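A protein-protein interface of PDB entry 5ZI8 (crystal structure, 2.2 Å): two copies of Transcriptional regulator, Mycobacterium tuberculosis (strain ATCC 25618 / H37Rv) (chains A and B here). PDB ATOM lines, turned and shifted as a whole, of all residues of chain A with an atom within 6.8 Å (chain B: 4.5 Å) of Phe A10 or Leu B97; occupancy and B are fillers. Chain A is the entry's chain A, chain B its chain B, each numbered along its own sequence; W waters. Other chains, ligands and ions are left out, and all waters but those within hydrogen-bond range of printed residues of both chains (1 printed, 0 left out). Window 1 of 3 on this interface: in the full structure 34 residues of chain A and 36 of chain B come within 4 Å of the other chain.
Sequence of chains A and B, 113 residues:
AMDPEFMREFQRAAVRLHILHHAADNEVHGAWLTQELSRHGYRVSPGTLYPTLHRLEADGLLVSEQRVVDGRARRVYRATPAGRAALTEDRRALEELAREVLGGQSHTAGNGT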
ATOM      1  N   GLU A   5     -32.875  -4.201 -35.996  1.00  0.00           N
ATOM      2  CA  GLU A   5     -33.873  -5.016 -35.347  1.00  0.00           C
ATOM      3  C   GLU A   5     -33.321  -6.378 -34.924  1.00  0.00           C
ATOM      4  O   GLU A   5     -33.568  -6.849 -33.832  1.00  0.00           O
ATOM      5  CB  GLU A   5     -35.098  -5.219 -36.242  1.00  0.00           C
ATOM      6  CG  GLU A   5     -36.207  -6.082 -35.612  1.00  0.00           C
ATOM      7  CD  GLU A   5     -36.659  -5.593 -34.193  1.00  0.00           C
ATOM      8  OE1 GLU A   5     -36.507  -4.394 -33.914  1.00  0.00           O
ATOM      9  OE2 GLU A   5     -37.172  -6.362 -33.322  1.00  0.00           O
ATOM     10  N   PHE A   6     -32.586  -7.015 -35.826  1.00  0.00           N
ATOM     11  CA  PHE A   6     -31.879  -8.211 -35.504  1.00  0.00           C
ATOM     12  C   PHE A   6     -30.970  -8.012 -34.322  1.00  0.00           C
ATOM     13  O   PHE A   6     -30.952  -8.836 -33.415  1.00  0.00           O
ATOM     14  CB  PHE A   6     -30.994  -8.692 -36.634  1.00  0.00           C
ATOM     15  CG  PHE A   6     -30.201  -9.901 -36.245  1.00  0.00           C
ATOM     16  CD1 PHE A   6     -30.792 -11.180 -36.270  1.00  0.00           C
ATOM     17  CD2 PHE A   6     -28.935  -9.776 -35.778  1.00  0.00           C
ATOM     18  CE1 PHE A   6     -30.081 -12.298 -35.901  1.00  0.00           C
ATOM     19  CE2 PHE A   6     -28.214 -10.878 -35.362  1.00  0.00           C
ATOM     20  CZ  PHE A   6     -28.774 -12.153 -35.441  1.00  0.00           C
ATOM     21  N   MET A   7     -30.167  -6.949 -34.348  1.00  0.00           N
ATOM     22  CA  MET A   7     -29.196  -6.730 -33.251  1.00  0.00           C
ATOM     23  C   MET A   7     -29.868  -6.561 -31.923  1.00  0.00           C
ATOM     24  O   MET A   7     -29.430  -7.121 -30.930  1.00  0.00           O
ATOM     25  CB  MET A   7     -28.306  -5.536 -33.529  1.00  0.00           C
ATOM     26  CG  MET A   7     -27.336  -5.795 -34.664  1.00  0.00           C
ATOM     27  SD  MET A   7     -26.217  -7.228 -34.498  1.00  0.00           S
ATOM     28  CE  MET A   7     -25.434  -7.042 -36.117  1.00  0.00           C
ATOM     29  N   ARG A   8     -30.969  -5.824 -31.934  1.00  0.00           N
ATOM     30  CA  ARG A   8     -31.788  -5.648 -30.755  1.00  0.00           C
ATOM     31  C   ARG A   8     -32.376  -6.951 -30.203  1.00  0.00           C
ATOM     32  O   ARG A   8     -32.195  -7.245 -29.060  1.00  0.00           O
ATOM     33  CB  ARG A   8     -32.885  -4.656 -31.108  1.00  0.00           C
ATOM     34  CG  ARG A   8     -33.684  -4.073 -29.978  1.00  0.00           C
ATOM     35  CD  ARG A   8     -34.451  -2.835 -30.449  1.00  0.00           C
ATOM     36  NE  ARG A   8     -34.945  -2.869 -31.845  1.00  0.00           N
ATOM     37  CZ  ARG A   8     -34.724  -1.924 -32.796  1.00  0.00           C
ATOM     38  NH1 ARG A   8     -33.952  -0.844 -32.597  1.00  0.00           N
ATOM     39  NH2 ARG A   8     -35.282  -2.052 -33.988  1.00  0.00           N
ATOM     40  N   GLU A   9     -33.058  -7.722 -31.044  1.00  0.00           N
ATOM     41  CA  GLU A   9     -33.600  -8.988 -30.619  1.00  0.00           C
ATOM     42  C   GLU A   9     -32.501  -9.917 -30.144  1.00  0.00           C
ATOM     43  O   GLU A   9     -32.618 -10.566 -29.127  1.00  0.00           O
ATOM     44  CB  GLU A   9     -34.306  -9.681 -31.788  1.00  0.00           C
ATOM     45  CG  GLU A   9     -35.592  -8.994 -32.272  1.00  0.00           C
ATOM     46  CD  GLU A   9     -36.065  -9.535 -33.649  1.00  0.00           C
ATOM     47  OE1 GLU A   9     -35.464 -10.494 -34.231  1.00  0.00           O
ATOM     48  OE2 GLU A   9     -37.043  -8.998 -34.214  1.00  0.00           O
ATOM     49  N   PHE A  10     -31.433  -9.988 -30.909  1.00  0.00           N
ATOM     50  CA  PHE A  10     -30.356 -10.893 -30.614  1.00  0.00           C
ATOM     51  C   PHE A  10     -29.621 -10.504 -29.344  1.00  0.00           C
ATOM     52  O   PHE A  10     -29.247 -11.380 -28.559  1.00  0.00           O
ATOM     53  CB  PHE A  10     -29.384 -10.902 -31.741  1.00  0.00           C
ATOM     54  CG  PHE A  10     -28.274 -11.907 -31.583  1.00  0.00           C
ATOM     55  CD1 PHE A  10     -28.490 -13.247 -31.870  1.00  0.00           C
ATOM     56  CD2 PHE A  10     -27.018 -11.516 -31.185  1.00  0.00           C
ATOM     57  CE1 PHE A  10     -27.461 -14.176 -31.750  1.00  0.00           C
ATOM     58  CE2 PHE A  10     -25.978 -12.438 -31.065  1.00  0.00           C
ATOM     59  CZ  PHE A  10     -26.206 -13.766 -31.335  1.00  0.00           C
ATOM     60  N   GLN A  11     -29.426  -9.215 -29.140  1.00  0.00           N
ATOM     61  CA  GLN A  11     -28.786  -8.794 -27.925  1.00  0.00           C
ATOM     62  C   GLN A  11     -29.631  -9.188 -26.709  1.00  0.00           C
ATOM     63  O   GLN A  11     -29.070  -9.471 -25.688  1.00  0.00           O
ATOM     64  CB  GLN A  11     -28.437  -7.287 -27.901  1.00  0.00           C
ATOM     65  CG  GLN A  11     -28.288  -6.756 -26.453  1.00  0.00           C
ATOM     66  CD  GLN A  11     -27.513  -5.476 -26.225  1.00  0.00           C
ATOM     67  OE1 GLN A  11     -26.679  -5.035 -27.033  1.00  0.00           O
ATOM     68  NE2 GLN A  11     -27.720  -4.923 -25.037  1.00  0.00           N
ATOM     69  N   ARG A  12     -30.954  -9.164 -26.789  1.00  0.00           N
ATOM     70  CA  ARG A  12     -31.763  -9.534 -25.612  1.00  0.00           C
ATOM     71  C   ARG A  12     -31.548 -10.989 -25.240  1.00  0.00           C
ATOM     72  O   ARG A  12     -31.450 -11.321 -24.051  1.00  0.00           O
ATOM     73  CB  ARG A  12     -33.243  -9.382 -25.861  1.00  0.00           C
ATOM     74  CG  ARG A  12     -33.694  -7.961 -26.086  1.00  0.00           C
ATOM     75  CD  ARG A  12     -35.175  -7.907 -26.401  1.00  0.00           C
ATOM     76  NE  ARG A  12     -35.889  -8.465 -25.245  1.00  0.00           N
ATOM     77  CZ  ARG A  12     -37.105  -9.019 -25.260  1.00  0.00           C
ATOM     78  NH1 ARG A  12     -37.837  -9.146 -26.397  1.00  0.00           N
ATOM     79  NH2 ARG A  12     -37.611  -9.468 -24.098  1.00  0.00           N
ATOM     80  N   ALA A  13     -31.460 -11.839 -26.270  1.00  0.00           N
ATOM     81  CA  ALA A  13     -31.195 -13.266 -26.076  1.00  0.00           C
ATOM     82  C   ALA A  13     -29.794 -13.478 -25.543  1.00  0.00           C
ATOM     83  O   ALA A  13     -29.603 -14.269 -24.626  1.00  0.00           O
ATOM     84  CB  ALA A  13     -31.405 -14.092 -27.347  1.00  0.00           C
ATOM     85  N   ALA A  14     -28.823 -12.760 -26.090  1.00  0.00           N
ATOM     86  CA  ALA A  14     -27.445 -12.967 -25.680  1.00  0.00           C
ATOM     87  C   ALA A  14     -27.172 -12.511 -24.239  1.00  0.00           C
ATOM     88  O   ALA A  14     -26.456 -13.153 -23.519  1.00  0.00           O
ATOM     89  CB  ALA A  14     -26.520 -12.245 -26.615  1.00  0.00           C
ATOM     90  N   VAL A  15     -27.809 -11.438 -23.831  1.00  0.00           N
ATOM     91  CA  VAL A  15     -27.672 -10.931 -22.480  1.00  0.00           C
ATOM     92  C   VAL A  15     -28.211 -11.992 -21.514  1.00  0.00           C
ATOM     93  O   VAL A  15     -27.535 -12.355 -20.535  1.00  0.00           O
ATOM     94  CB  VAL A  15     -28.370  -9.559 -22.324  1.00  0.00           C
ATOM     95  CG1 VAL A  15     -28.623  -9.192 -20.885  1.00  0.00           C
ATOM     96  CG2 VAL A  15     -27.550  -8.459 -23.004  1.00  0.00           C
ATOM     97  N   LEU A  17     -28.546 -15.163 -21.892  1.00  0.00           N
ATOM     98  CA  LEU A  17     -27.661 -16.286 -21.857  1.00  0.00           C
ATOM     99  C   LEU A  17     -26.386 -16.040 -21.057  1.00  0.00           C
ATOM    100  O   LEU A  17     -25.934 -16.917 -20.284  1.00  0.00           O
ATOM    101  CB  LEU A  17     -27.294 -16.605 -23.275  1.00  0.00           C
ATOM    102  CG  LEU A  17     -26.507 -17.859 -23.601  1.00  0.00           C
ATOM    103  CD1 LEU A  17     -27.198 -19.043 -23.007  1.00  0.00           C
ATOM    104  CD2 LEU A  17     -26.472 -17.984 -25.118  1.00  0.00           C
ATOM    105  N   HIS A  18     -25.810 -14.841 -21.227  1.00  0.00           N
ATOM    106  CA  HIS A  18     -24.639 -14.473 -20.458  1.00  0.00           C
ATOM    107  C   HIS A  18     -24.908 -14.364 -18.977  1.00  0.00           C
ATOM    108  O   HIS A  18     -24.047 -14.671 -18.194  1.00  0.00           O
ATOM    109  CB  HIS A  18     -24.050 -13.132 -20.904  1.00  0.00           C
ATOM    110  CG  HIS A  18     -22.957 -13.256 -21.906  1.00  0.00           C
ATOM    111  ND1 HIS A  18     -23.140 -12.945 -23.242  1.00  0.00           N
ATOM    112  CD2 HIS A  18     -21.668 -13.651 -21.781  1.00  0.00           C
ATOM    113  CE1 HIS A  18     -22.009 -13.119 -23.894  1.00  0.00           C
ATOM    114  NE2 HIS A  18     -21.106 -13.568 -23.041  1.00  0.00           N
ATOM    115  N   TYR A  42     -21.878  -5.726 -24.552  1.00  0.00           N
ATOM    116  CA  TYR A  42     -23.316  -5.489 -24.472  1.00  0.00           C
ATOM    117  C   TYR A  42     -23.634  -4.198 -23.725  1.00  0.00           C
ATOM    118  O   TYR A  42     -23.216  -3.983 -22.622  1.00  0.00           O
ATOM    119  CB  TYR A  42     -24.043  -6.726 -23.890  1.00  0.00           C
ATOM    120  CG  TYR A  42     -23.786  -7.960 -24.742  1.00  0.00           C
ATOM    121  CD1 TYR A  42     -24.469  -8.184 -25.950  1.00  0.00           C
ATOM    122  CD2 TYR A  42     -22.772  -8.842 -24.401  1.00  0.00           C
ATOM    123  CE1 TYR A  42     -24.146  -9.274 -26.774  1.00  0.00           C
ATOM    124  CE2 TYR A  42     -22.444  -9.932 -25.194  1.00  0.00           C
ATOM    125  CZ  TYR A  42     -23.117 -10.148 -26.379  1.00  0.00           C
ATOM    126  OH  TYR A  42     -22.763 -11.241 -27.150  1.00  0.00           O
ATOM    127  N   LEU A  94     -28.301 -22.193 -29.667  1.00  0.00           N
ATOM    128  CA  LEU A  94     -27.289 -21.368 -30.319  1.00  0.00           C
ATOM    129  C   LEU A  94     -26.396 -22.203 -31.218  1.00  0.00           C
ATOM    130  O   LEU A  94     -26.096 -21.790 -32.327  1.00  0.00           O
ATOM    131  CB  LEU A  94     -26.475 -20.637 -29.279  1.00  0.00           C
ATOM    132  CG  LEU A  94     -25.271 -19.814 -29.682  1.00  0.00           C
ATOM    133  CD1 LEU A  94     -25.739 -18.620 -30.477  1.00  0.00           C
ATOM    134  CD2 LEU A  94     -24.586 -19.330 -28.401  1.00  0.00           C
ATOM    135  N   LEU A  97     -28.225 -22.963 -34.519  1.00  0.00           N
ATOM    136  CA  LEU A  97     -28.336 -21.895 -35.436  1.00  0.00           C
ATOM    137  C   LEU A  97     -26.996 -21.614 -36.062  1.00  0.00           C
ATOM    138  O   LEU A  97     -26.909 -21.378 -37.245  1.00  0.00           O
ATOM    139  CB  LEU A  97     -28.902 -20.653 -34.778  1.00  0.00           C
ATOM    140  CG  LEU A  97     -29.122 -19.454 -35.732  1.00  0.00           C
ATOM    141  CD1 LEU A  97     -30.082 -19.753 -36.893  1.00  0.00           C
ATOM    142  CD2 LEU A  97     -29.538 -18.275 -34.841  1.00  0.00           C
ATOM    143  N   ALA B  13     -34.993 -13.757 -33.555  1.00  0.00           N
ATOM    144  CA  ALA B  13     -33.694 -13.437 -34.163  1.00  0.00           C
ATOM    145  C   ALA B  13     -33.308 -14.497 -35.175  1.00  0.00           C
ATOM    146  O   ALA B  13     -32.874 -14.157 -36.274  1.00  0.00           O
ATOM    147  CB  ALA B  13     -32.605 -13.254 -33.099  1.00  0.00           C
ATOM    148  N   ALA B  93     -22.072 -11.570 -35.527  1.00  0.00           N
ATOM    149  CA  ALA B  93     -22.547 -11.499 -34.155  1.00  0.00           C
ATOM    150  C   ALA B  93     -22.811 -12.922 -33.580  1.00  0.00           C
ATOM    151  O   ALA B  93     -22.471 -13.221 -32.413  1.00  0.00           O
ATOM    152  CB  ALA B  93     -23.835 -10.652 -34.095  1.00  0.00           C
ATOM    153  N   LEU B  94     -23.415 -13.779 -34.410  1.00  0.00           N
ATOM    154  CA  LEU B  94     -23.684 -15.152 -33.986  1.00  0.00           C
ATOM    155  C   LEU B  94     -22.391 -15.914 -33.732  1.00  0.00           C
ATOM    156  O   LEU B  94     -22.305 -16.618 -32.727  1.00  0.00           O
ATOM    157  CB  LEU B  94     -24.514 -15.877 -35.031  1.00  0.00           C
ATOM    158  CG  LEU B  94     -24.830 -17.334 -34.830  1.00  0.00           C
ATOM    159  CD1 LEU B  94     -25.751 -17.506 -33.645  1.00  0.00           C
ATOM    160  CD2 LEU B  94     -25.465 -17.898 -36.071  1.00  0.00           C
ATOM    161  N   GLU B  95     -21.408 -15.771 -34.623  1.00  0.00           N
ATOM    162  CA  GLU B  95     -20.127 -16.445 -34.435  1.00  0.00           C
ATOM    163  C   GLU B  95     -19.501 -16.006 -33.142  1.00  0.00           C
ATOM    164  O   GLU B  95     -18.954 -16.828 -32.445  1.00  0.00           O
ATOM    165  CB  GLU B  95     -19.131 -16.132 -35.536  1.00  0.00           C
ATOM    166  CG  GLU B  95     -18.232 -17.284 -36.035  1.00  0.00           C
ATOM    167  CD  GLU B  95     -17.918 -17.159 -37.544  1.00  0.00           C
ATOM    168  OE1 GLU B  95     -18.550 -16.327 -38.240  1.00  0.00           O
ATOM    169  OE2 GLU B  95     -17.046 -17.857 -38.076  1.00  0.00           O
ATOM    170  N   GLU B  96     -19.566 -14.723 -32.830  1.00  0.00           N
ATOM    171  CA  GLU B  96     -18.909 -14.242 -31.635  1.00  0.00           C
ATOM    172  C   GLU B  96     -19.573 -14.795 -30.391  1.00  0.00           C
ATOM    173  O   GLU B  96     -18.860 -15.213 -29.470  1.00  0.00           O
ATOM    174  CB  GLU B  96     -18.878 -12.710 -31.566  1.00  0.00           C
ATOM    175  CG  GLU B  96     -18.005 -12.117 -32.683  1.00  0.00           C
ATOM    176  CD  GLU B  96     -17.821 -10.597 -32.609  1.00  0.00           C
ATOM    177  OE1 GLU B  96     -17.841 -10.062 -31.466  1.00  0.00           O
ATOM    178  OE2 GLU B  96     -17.610  -9.968 -33.692  1.00  0.00           O
ATOM    179  N   LEU B  97     -20.921 -14.843 -30.358  1.00  0.00           N
ATOM    180  CA  LEU B  97     -21.566 -15.324 -29.187  1.00  0.00           C
ATOM    181  C   LEU B  97     -21.281 -16.781 -29.027  1.00  0.00           C
ATOM    182  O   LEU B  97     -21.058 -17.233 -27.927  1.00  0.00           O
ATOM    183  CB  LEU B  97     -23.052 -15.078 -29.230  1.00  0.00           C
ATOM    184  CG  LEU B  97     -23.835 -15.497 -27.975  1.00  0.00           C
ATOM    185  CD1 LEU B  97     -23.375 -14.768 -26.713  1.00  0.00           C
ATOM    186  CD2 LEU B  97     -25.318 -15.247 -28.134  1.00  0.00           C
ATOM    187  N   ALA B  98     -21.302 -17.516 -30.140  1.00  0.00           N
ATOM    188  CA  ALA B  98     -20.951 -18.959 -30.153  1.00  0.00           C
ATOM    189  C   ALA B  98     -19.599 -19.219 -29.519  1.00  0.00           C
ATOM    190  O   ALA B  98     -19.513 -20.023 -28.573  1.00  0.00           O
ATOM    191  CB  ALA B  98     -20.986 -19.553 -31.552  1.00  0.00           C
ATOM    192  N   ARG B  99     -18.567 -18.531 -30.009  1.00  0.00           N
ATOM    193  CA  ARG B  99     -17.217 -18.644 -29.408  1.00  0.00           C
ATOM    194  C   ARG B  99     -17.146 -18.347 -27.899  1.00  0.00           C
ATOM    195  O   ARG B  99     -16.508 -19.085 -27.171  1.00  0.00           O
ATOM    196  CB  ARG B  99     -16.196 -17.770 -30.140  1.00  0.00           C
ATOM    197  CG  ARG B  99     -15.740 -18.298 -31.507  1.00  0.00           C
ATOM    198  N   GLU B 100     -17.797 -17.281 -27.449  1.00  0.00           N
ATOM    199  CA  GLU B 100     -17.832 -16.893 -26.024  1.00  0.00           C
ATOM    200  C   GLU B 100     -18.511 -17.906 -25.055  1.00  0.00           C
ATOM    201  O   GLU B 100     -18.000 -18.193 -23.962  1.00  0.00           O
ATOM    202  CB  GLU B 100     -18.606 -15.564 -25.844  1.00  0.00           C
ATOM    203  CG  GLU B 100     -18.039 -14.280 -26.374  1.00  0.00           C
ATOM    204  CD  GLU B 100     -19.019 -13.129 -26.104  1.00  0.00           C
ATOM    205  OE1 GLU B 100     -20.045 -13.034 -26.829  1.00  0.00           O
ATOM    206  OE2 GLU B 100     -18.780 -12.333 -25.151  1.00  0.00           O
ATOM    207  N   VAL B 101     -19.688 -18.395 -25.444  1.00  0.00           N
ATOM    208  CA  VAL B 101     -20.613 -19.056 -24.510  1.00  0.00           C
ATOM    209  C   VAL B 101     -20.502 -20.582 -24.580  1.00  0.00           C
ATOM    210  O   VAL B 101     -21.023 -21.281 -23.723  1.00  0.00           O
ATOM    211  CB  VAL B 101     -22.053 -18.562 -24.736  1.00  0.00           C
HETATM  212  O   HOH W   1     -22.700 -11.256 -30.322  1.00  0.00           O
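Printed residues of chain A that touch a printed residue of chain B: Phe A6, Glu A9, Phe A10, Ala A14, His A18, Tyr A42, Leu A94 and Leu A97. Hydrophobic or aromatic side chains of chain A that line the printed part of chain B: Phe A6, Phe A10, Ala A14, His A18, Tyr A42, Leu A94 and Leu A97. Printed residues of chain B that touch a printed residue of chain A: Ala B13, Ala B93, Leu B94, Leu B97 and Glu B100. Among the printed residues, 13 pairs touch across the chains. Among the printed residues, no Asp or Glu carboxylate lies within 4 Å of a Lys or Arg side-chain nitrogen of the other chain.
The side-chain carboxylate of Glu B100 is in hydrogen-bond range of a ring nitrogen (NE2) of His A18 (3.4 Å). OH of Tyr A42 sits at hydrogen-bond distance from OE1 of Glu B100. The side-chain carboxylate of Glu A9 sits at hydrogen-bond distance from the backbone NH of Ala B13 (3.4 Å).
Leu B94 touches its own counterpart, Leu A94. Leu A94 touches Leu B97, and with the chains exchanged Leu A97 touches Leu B94. Of the 13 pairs that touch across the chains among the printed residues, 3 have their exchanged pair printed and touching as well.
Water W1 lies within hydrogen-bond range of O of Ala B93 and OH of Tyr A42.
Of chain B, only Ala B93, Leu B94 and Leu B97 come within 4 Å of Phe A10. Of chain A, only Phe A10 (3.6 Å), Ala A14 (3.6 Å), His A18 (3.5 Å), Tyr A42 (3.6 Å) and Leu A94 (3.9 Å) come within 4 Å of Leu B97. Of the printed residues of chain B, Leu A94 touches Leu B94 (3.4 Å) and Leu B97 (3.9 Å). Of the printed residues of chain B, His A18 touches Leu B97 and Glu B100. Of the printed residues of chain B, Glu A9 touches Ala B13 (3.4 Å). Of the printed residues of chain A, Glu B100 touches His A18 and Tyr A42. Ala A13 touches none of the printed residues of chain B. The nearest residue of chain B that does not touch Phe A10 is Ala B13 (4.1 Å). The nearest residue of chain A that does not touch Leu B97 is Leu A17 (4.2 Å).
Ala B13 touches Phe A6 (O to CE1, 3.4 Å). O of Ala B93 touches CE2 of Phe A10, at 3.8 Å. Leu B94 touches Phe A10 (CA to CZ, 3.9 Å). Phe A10 touches Leu B97 (CZ to CD2, 3.6 Å). CB of Ala A14 touches CD2 of Leu B97, at 3.6 Å. His A18 touches Leu B97 (CE1 to CD1, 3.5 Å). Tyr A42 touches Leu B97. Leu B94 touches Leu A94 (CD1 to CD1, 3.4 Å). Leu A94 touches Leu B97. Leu B94 touches Leu A97.
The backbone carbonyl oxygen of Ala A14 lies within hydrogen-bond range of a ring nitrogen (ND1) of His A18, 3.3 Å away.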
